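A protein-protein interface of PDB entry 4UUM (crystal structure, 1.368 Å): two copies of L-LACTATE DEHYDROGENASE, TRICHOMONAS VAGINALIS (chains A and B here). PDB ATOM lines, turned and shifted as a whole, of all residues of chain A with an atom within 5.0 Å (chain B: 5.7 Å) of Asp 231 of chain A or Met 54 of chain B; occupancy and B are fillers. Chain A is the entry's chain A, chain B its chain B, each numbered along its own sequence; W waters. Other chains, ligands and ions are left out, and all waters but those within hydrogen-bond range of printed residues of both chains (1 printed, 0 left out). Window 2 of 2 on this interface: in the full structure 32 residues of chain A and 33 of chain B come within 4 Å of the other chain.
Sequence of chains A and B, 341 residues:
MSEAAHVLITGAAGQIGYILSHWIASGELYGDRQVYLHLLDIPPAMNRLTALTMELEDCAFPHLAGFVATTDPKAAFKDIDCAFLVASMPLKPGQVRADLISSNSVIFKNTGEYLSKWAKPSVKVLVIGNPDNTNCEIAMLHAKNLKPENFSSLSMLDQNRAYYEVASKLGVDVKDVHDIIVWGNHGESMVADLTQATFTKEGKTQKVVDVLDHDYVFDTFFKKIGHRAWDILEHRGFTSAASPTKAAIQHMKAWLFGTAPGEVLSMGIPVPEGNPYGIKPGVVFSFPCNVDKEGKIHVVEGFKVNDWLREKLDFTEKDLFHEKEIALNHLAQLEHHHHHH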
ATOM      1  N   HIS A 227     -29.341 -36.995  25.660  1.00  0.00           N
ATOM      2  CA  HIS A 227     -29.508 -35.814  26.515  1.00  0.00           C
ATOM      3  C   HIS A 227     -28.913 -34.543  25.903  1.00  0.00           C
ATOM      4  O   HIS A 227     -28.902 -33.482  26.540  1.00  0.00           O
ATOM      5  CB  HIS A 227     -28.885 -36.059  27.889  1.00  0.00           C
ATOM      6  CG  HIS A 227     -29.681 -36.985  28.757  1.00  0.00           C
ATOM      7  ND1 HIS A 227     -29.623 -38.358  28.633  1.00  0.00           N
ATOM      8  CD2 HIS A 227     -30.557 -36.735  29.759  1.00  0.00           C
ATOM      9  CE1 HIS A 227     -30.423 -38.913  29.526  1.00  0.00           C
ATOM     10  NE2 HIS A 227     -31.002 -37.951  30.222  1.00  0.00           N
ATOM     11  N   ARG A 228     -28.444 -34.649  24.664  1.00  0.00           N
ATOM     12  CA  ARG A 228     -27.758 -33.544  23.999  1.00  0.00           C
ATOM     13  C   ARG A 228     -28.633 -32.293  23.819  1.00  0.00           C
ATOM     14  O   ARG A 228     -28.196 -31.162  24.075  1.00  0.00           O
ATOM     15  CB  ARG A 228     -27.250 -34.007  22.629  1.00  0.00           C
ATOM     16  CG  ARG A 228     -26.471 -32.949  21.878  1.00  0.00           C
ATOM     17  CD  ARG A 228     -25.232 -32.530  22.632  1.00  0.00           C
ATOM     18  NE  ARG A 228     -24.279 -31.893  21.730  1.00  0.00           N
ATOM     19  CZ  ARG A 228     -23.030 -31.581  22.048  1.00  0.00           C
ATOM     20  NH1 ARG A 228     -22.562 -31.801  23.275  1.00  0.00           N
ATOM     21  NH2 ARG A 228     -22.253 -31.014  21.140  1.00  0.00           N
ATOM     22  N   ALA A 229     -29.863 -32.501  23.372  1.00  0.00           N
ATOM     23  CA  ALA A 229     -30.785 -31.405  23.116  1.00  0.00           C
ATOM     24  C   ALA A 229     -31.109 -30.668  24.414  1.00  0.00           C
ATOM     25  O   ALA A 229     -31.143 -29.435  24.448  1.00  0.00           O
ATOM     26  CB  ALA A 229     -32.047 -31.939  22.481  1.00  0.00           C
ATOM     27  N   TRP A 230     -31.345 -31.436  25.472  1.00  0.00           N
ATOM     28  CA  TRP A 230     -31.612 -30.903  26.800  1.00  0.00           C
ATOM     29  C   TRP A 230     -30.446 -30.044  27.280  1.00  0.00           C
ATOM     30  O   TRP A 230     -30.636 -28.938  27.789  1.00  0.00           O
ATOM     31  CB  TRP A 230     -31.851 -32.066  27.772  1.00  0.00           C
ATOM     32  CG  TRP A 230     -32.058 -31.633  29.186  1.00  0.00           C
ATOM     33  CD1 TRP A 230     -31.209 -31.829  30.240  1.00  0.00           C
ATOM     34  CD2 TRP A 230     -33.185 -30.921  29.704  1.00  0.00           C
ATOM     35  NE1 TRP A 230     -31.741 -31.283  31.383  1.00  0.00           N
ATOM     36  CE2 TRP A 230     -32.954 -30.721  31.082  1.00  0.00           C
ATOM     37  CE3 TRP A 230     -34.369 -30.434  29.140  1.00  0.00           C
ATOM     38  CZ2 TRP A 230     -33.864 -30.053  31.901  1.00  0.00           C
ATOM     39  CZ3 TRP A 230     -35.271 -29.772  29.957  1.00  0.00           C
ATOM     40  CH2 TRP A 230     -35.014 -29.588  31.321  1.00  0.00           C
ATOM     41  N   ASP A 231     -29.235 -30.557  27.097  1.00  0.00           N
ATOM     42  CA  ASP A 231     -28.036 -29.867  27.546  1.00  0.00           C
ATOM     43  C   ASP A 231     -27.902 -28.507  26.840  1.00  0.00           C
ATOM     44  O   ASP A 231     -27.555 -27.485  27.453  1.00  0.00           O
ATOM     45  CB  ASP A 231     -26.821 -30.757  27.273  1.00  0.00           C
ATOM     46  CG  ASP A 231     -25.641 -30.435  28.165  1.00  0.00           C
ATOM     47  OD1 ASP A 231     -25.833 -29.727  29.177  1.00  0.00           O
ATOM     48  OD2 ASP A 231     -24.522 -30.905  27.856  1.00  0.00           O
ATOM     49  N   ILE A 232     -28.195 -28.495  25.544  1.00  0.00           N
ATOM     50  CA  ILE A 232     -28.182 -27.258  24.781  1.00  0.00           C
ATOM     51  C   ILE A 232     -29.252 -26.280  25.262  1.00  0.00           C
ATOM     52  O   ILE A 232     -28.978 -25.093  25.426  1.00  0.00           O
ATOM     53  CB  ILE A 232     -28.351 -27.547  23.285  1.00  0.00           C
ATOM     54  CG1 ILE A 232     -27.077 -28.211  22.767  1.00  0.00           C
ATOM     55  CG2 ILE A 232     -28.631 -26.262  22.499  1.00  0.00           C
ATOM     56  CD1 ILE A 232     -27.177 -28.733  21.385  1.00  0.00           C
ATOM     57  N   LEU A 233     -30.461 -26.776  25.492  1.00  0.00           N
ATOM     58  CA  LEU A 233     -31.551 -25.944  26.006  1.00  0.00           C
ATOM     59  C   LEU A 233     -31.176 -25.301  27.345  1.00  0.00           C
ATOM     60  O   LEU A 233     -31.456 -24.125  27.589  1.00  0.00           O
ATOM     61  CB  LEU A 233     -32.828 -26.780  26.163  1.00  0.00           C
ATOM     62  CG  LEU A 233     -34.026 -26.072  26.807  1.00  0.00           C
ATOM     63  CD1 LEU A 233     -34.391 -24.802  26.034  1.00  0.00           C
ATOM     64  CD2 LEU A 233     -35.219 -27.011  26.908  1.00  0.00           C
ATOM     65  N   GLU A 234     -30.527 -26.083  28.203  1.00  0.00           N
ATOM     66  CA  GLU A 234     -30.051 -25.600  29.495  1.00  0.00           C
ATOM     67  C   GLU A 234     -29.055 -24.451  29.362  1.00  0.00           C
ATOM     68  O   GLU A 234     -29.106 -23.495  30.135  1.00  0.00           O
ATOM     69  CB  GLU A 234     -29.399 -26.748  30.264  1.00  0.00           C
ATOM     70  CG  GLU A 234     -30.380 -27.807  30.734  1.00  0.00           C
ATOM     71  CD  GLU A 234     -31.242 -27.329  31.880  1.00  0.00           C
ATOM     72  OE1 GLU A 234     -30.682 -27.013  32.949  1.00  0.00           O
ATOM     73  OE2 GLU A 234     -32.478 -27.265  31.710  1.00  0.00           O
ATOM     74  N   HIS A 235     -28.154 -24.545  28.381  1.00  0.00           N
ATOM     75  CA  HIS A 235     -27.106 -23.537  28.193  1.00  0.00           C
ATOM     76  C   HIS A 235     -27.608 -22.327  27.395  1.00  0.00           C
ATOM     77  O   HIS A 235     -27.253 -21.181  27.701  1.00  0.00           O
ATOM     78  CB  HIS A 235     -25.894 -24.147  27.468  1.00  0.00           C
ATOM     79  CG  HIS A 235     -25.037 -25.034  28.324  1.00  0.00           C
ATOM     80  ND1 HIS A 235     -25.377 -26.335  28.638  1.00  0.00           N
ATOM     81  CD2 HIS A 235     -23.836 -24.811  28.909  1.00  0.00           C
ATOM     82  CE1 HIS A 235     -24.428 -26.868  29.388  1.00  0.00           C
ATOM     83  NE2 HIS A 235     -23.482 -25.964  29.568  1.00  0.00           N
ATOM     84  N   LEU B  49     -22.365 -19.144  24.922  1.00  0.00           N
ATOM     85  CA  LEU B  49     -21.320 -19.470  23.967  1.00  0.00           C
ATOM     86  C   LEU B  49     -21.066 -20.981  23.918  1.00  0.00           C
ATOM     87  O   LEU B  49     -20.843 -21.554  22.851  1.00  0.00           O
ATOM     88  CB  LEU B  49     -20.037 -18.713  24.282  1.00  0.00           C
ATOM     89  CG  LEU B  49     -18.956 -18.825  23.212  1.00  0.00           C
ATOM     90  CD1 LEU B  49     -19.492 -18.510  21.813  1.00  0.00           C
ATOM     91  CD2 LEU B  49     -17.838 -17.880  23.563  1.00  0.00           C
ATOM     92  N   THR B  50     -21.120 -21.637  25.066  1.00  0.00           N
ATOM     93  CA  THR B  50     -20.972 -23.082  25.104  1.00  0.00           C
ATOM     94  C   THR B  50     -22.097 -23.730  24.285  1.00  0.00           C
ATOM     95  O   THR B  50     -21.853 -24.661  23.512  1.00  0.00           O
ATOM     96  CB  THR B  50     -20.955 -23.611  26.551  1.00  0.00           C
ATOM     97  OG1 THR B  50     -19.778 -23.132  27.221  1.00  0.00           O
ATOM     98  CG2 THR B  50     -20.945 -25.142  26.603  1.00  0.00           C
ATOM     99  N   ALA B  51     -23.319 -23.224  24.444  1.00  0.00           N
ATOM    100  CA  ALA B  51     -24.451 -23.724  23.664  1.00  0.00           C
ATOM    101  C   ALA B  51     -24.173 -23.583  22.172  1.00  0.00           C
ATOM    102  O   ALA B  51     -24.474 -24.488  21.393  1.00  0.00           O
ATOM    103  CB  ALA B  51     -25.709 -22.977  24.014  1.00  0.00           C
ATOM    104  N   LEU B  52     -23.616 -22.445  21.764  1.00  0.00           N
ATOM    105  CA  LEU B  52     -23.278 -22.228  20.357  1.00  0.00           C
ATOM    106  C   LEU B  52     -22.315 -23.300  19.890  1.00  0.00           C
ATOM    107  O   LEU B  52     -22.507 -23.895  18.834  1.00  0.00           O
ATOM    108  CB  LEU B  52     -22.667 -20.834  20.121  1.00  0.00           C
ATOM    109  CG  LEU B  52     -21.831 -20.691  18.832  1.00  0.00           C
ATOM    110  CD1 LEU B  52     -22.679 -20.980  17.625  1.00  0.00           C
ATOM    111  CD2 LEU B  52     -21.219 -19.310  18.716  1.00  0.00           C
ATOM    112  N   THR B  53     -21.253 -23.518  20.648  1.00  0.00           N
ATOM    113  CA  THR B  53     -20.242 -24.468  20.206  1.00  0.00           C
ATOM    114  C   THR B  53     -20.799 -25.892  20.151  1.00  0.00           C
ATOM    115  O   THR B  53     -20.402 -26.669  19.289  1.00  0.00           O
ATOM    116  CB  THR B  53     -18.929 -24.417  21.022  1.00  0.00           C
ATOM    117  OG1 THR B  53     -19.142 -24.844  22.374  1.00  0.00           O
ATOM    118  CG2 THR B  53     -18.333 -22.999  20.991  1.00  0.00           C
ATOM    119  N   MET B  54     -21.720 -26.231  21.045  1.00  0.00           N
ATOM    120  CA  MET B  54     -22.350 -27.552  21.010  1.00  0.00           C
ATOM    121  C   MET B  54     -23.124 -27.725  19.698  1.00  0.00           C
ATOM    122  O   MET B  54     -23.091 -28.776  19.077  1.00  0.00           O
ATOM    123  CB  MET B  54     -23.275 -27.742  22.214  1.00  0.00           C
ATOM    124  CG  MET B  54     -22.571 -27.899  23.544  1.00  0.00           C
ATOM    125  SD  MET B  54     -23.701 -27.777  24.952  1.00  0.00           S
ATOM    126  CE  MET B  54     -24.468 -29.370  24.864  1.00  0.00           C
ATOM    127  N   GLU B  55     -23.825 -26.686  19.268  1.00  0.00           N
ATOM    128  CA  GLU B  55     -24.518 -26.740  17.979  1.00  0.00           C
ATOM    129  C   GLU B  55     -23.574 -26.793  16.801  1.00  0.00           C
ATOM    130  O   GLU B  55     -23.841 -27.530  15.864  1.00  0.00           O
ATOM    131  CB  GLU B  55     -25.534 -25.612  17.829  1.00  0.00           C
ATOM    132  CG  GLU B  55     -26.790 -25.840  18.643  1.00  0.00           C
ATOM    133  CD  GLU B  55     -27.970 -25.067  18.143  1.00  0.00           C
ATOM    134  OE1 GLU B  55     -28.539 -25.480  17.115  1.00  0.00           O
ATOM    135  OE2 GLU B  55     -28.321 -24.027  18.765  1.00  0.00           O
ATOM    136  N   LEU B  56     -22.463 -26.060  16.847  1.00  0.00           N
ATOM    137  CA  LEU B  56     -21.451 -26.184  15.799  1.00  0.00           C
ATOM    138  C   LEU B  56     -20.974 -27.632  15.710  1.00  0.00           C
ATOM    139  O   LEU B  56     -20.896 -28.197  14.611  1.00  0.00           O
ATOM    140  CB  LEU B  56     -20.244 -25.282  16.055  1.00  0.00           C
ATOM    141  CG  LEU B  56     -20.464 -23.769  15.965  1.00  0.00           C
ATOM    142  CD1 LEU B  56     -19.197 -23.018  16.418  1.00  0.00           C
ATOM    143  CD2 LEU B  56     -20.825 -23.401  14.536  1.00  0.00           C
ATOM    144  N   GLU B  57     -20.652 -28.212  16.861  1.00  0.00           N
ATOM    145  CA  GLU B  57     -20.236 -29.622  16.905  1.00  0.00           C
ATOM    146  C   GLU B  57     -21.281 -30.531  16.270  1.00  0.00           C
ATOM    147  O   GLU B  57     -20.942 -31.423  15.479  1.00  0.00           O
ATOM    148  CB  GLU B  57     -19.978 -30.048  18.352  1.00  0.00           C
ATOM    149  CG  GLU B  57     -18.758 -29.377  18.963  1.00  0.00           C
ATOM    150  CD  GLU B  57     -18.576 -29.685  20.436  1.00  0.00           C
ATOM    151  OE1 GLU B  57     -19.545 -30.151  21.069  1.00  0.00           O
ATOM    152  OE2 GLU B  57     -17.450 -29.485  20.947  1.00  0.00           O
ATOM    153  N   ASP B  58     -22.539 -30.261  16.583  1.00  0.00           N
ATOM    154  CA  ASP B  58     -23.646 -31.118  16.163  1.00  0.00           C
ATOM    155  C   ASP B  58     -24.006 -30.970  14.684  1.00  0.00           C
ATOM    156  O   ASP B  58     -24.917 -31.659  14.189  1.00  0.00           O
ATOM    157  CB  ASP B  58     -24.899 -30.828  16.998  1.00  0.00           C
ATOM    158  CG  ASP B  58     -24.780 -31.312  18.417  1.00  0.00           C
ATOM    159  OD1 ASP B  58     -23.774 -31.979  18.749  1.00  0.00           O
ATOM    160  OD2 ASP B  58     -25.720 -31.049  19.198  1.00  0.00           O
ATOM    161  N   CYS B  59     -23.295 -30.106  13.976  1.00  0.00           N
ATOM    162  CA  CYS B  59     -23.441 -30.007  12.524  1.00  0.00           C
ATOM    163  C   CYS B  59     -22.453 -30.907  11.786  1.00  0.00           C
ATOM    164  O   CYS B  59     -22.608 -31.123  10.588  1.00  0.00           O
ATOM    165  CB  CYS B  59     -23.224 -28.557  12.067  1.00  0.00           C
ATOM    166  SG  CYS B  59     -24.571 -27.462  12.537  1.00  0.00           S
HETATM  167  O   HOH W   1     -19.754 -31.098  23.553  1.00  0.00           O
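Printed residues of chain B that touch a printed residue of chain A: Thr 50, Ala 51, Met 54, Glu 57 and Asp 58. Among the printed residues, 8 pairs touch across the chains.
ND1 of His 235 of chain A sits at hydrogen-bond distance from O of Asp 231 of chain A, at 2.7 Å. The side-chain hydroxyl (OG1) of Thr 53 of chain B sits at hydrogen-bond distance from the backbone carbonyl oxygen (O) of Thr 50 of chain B (2.9 Å).
Of chain B, only Met 54 comes within 4 Å of Asp 231 of chain A. Of the printed residues of chain B, Ile 232 of chain A touches Met 54 (3.5 Å) and Asp 58 (3.5 Å). Printed residues of chain B within 4 Å of His 235 of chain A: Thr 50 (3.7 Å) and Ala 51 (3.7 Å). Leu 49 of chain B touches none of the printed residues of chain A. Of the printed residues of chain A, Met 54 of chain B touches Arg 228, Asp 231 and Ile 232. Printed residues of chain A within 4 Å of Asp 58 of chain B: Arg 228 (3.0 Å) and Ile 232 (3.5 Å). The nearest residue of chain A that does not touch Met 54 of chain B is His 235 of chain A (4.3 Å).
No position is printed for both chains. Of the 8 pairs that touch across the chains among the printed residues, none has its exchanged pair printed and touching as well.
The guanidinium group (NH2) of Arg 228 of chain A sits at hydrogen-bond distance from the backbone carbonyl oxygen (O) of Met 54 of chain B (3.2 Å). The side-chain carboxylate (OE1) of Glu 57 of chain B is in salt-bridge range of the guanidinium group (NH2) of Arg 228 of chain A (2.8 Å). The guanidinium group of Arg 228 of chain A lies within salt-bridge range of the side-chain carboxylate of Asp 58 of chain B.
Water W1 bridges OE1 of Glu 57 of chain B (2.7 Å) and NH1 of Arg 228 of chain A (2.9 Å).
CE of Met 54 of chain B touches OD2 of Asp 231 of chain A (3.4 Å). Ile 232 of chain A touches Met 54 of chain B (CG1 to CE, 3.5 Å). OD2 of Asp 58 of chain B touches CD1 of Ile 232 of chain A, at 3.5 Å. Thr 50 of chain B touches His 235 of chain A (CG2 to CD2, 3.7 Å). Ala 51 of chain B touches His 235 of chain A (CB to CB, 3.7 Å).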
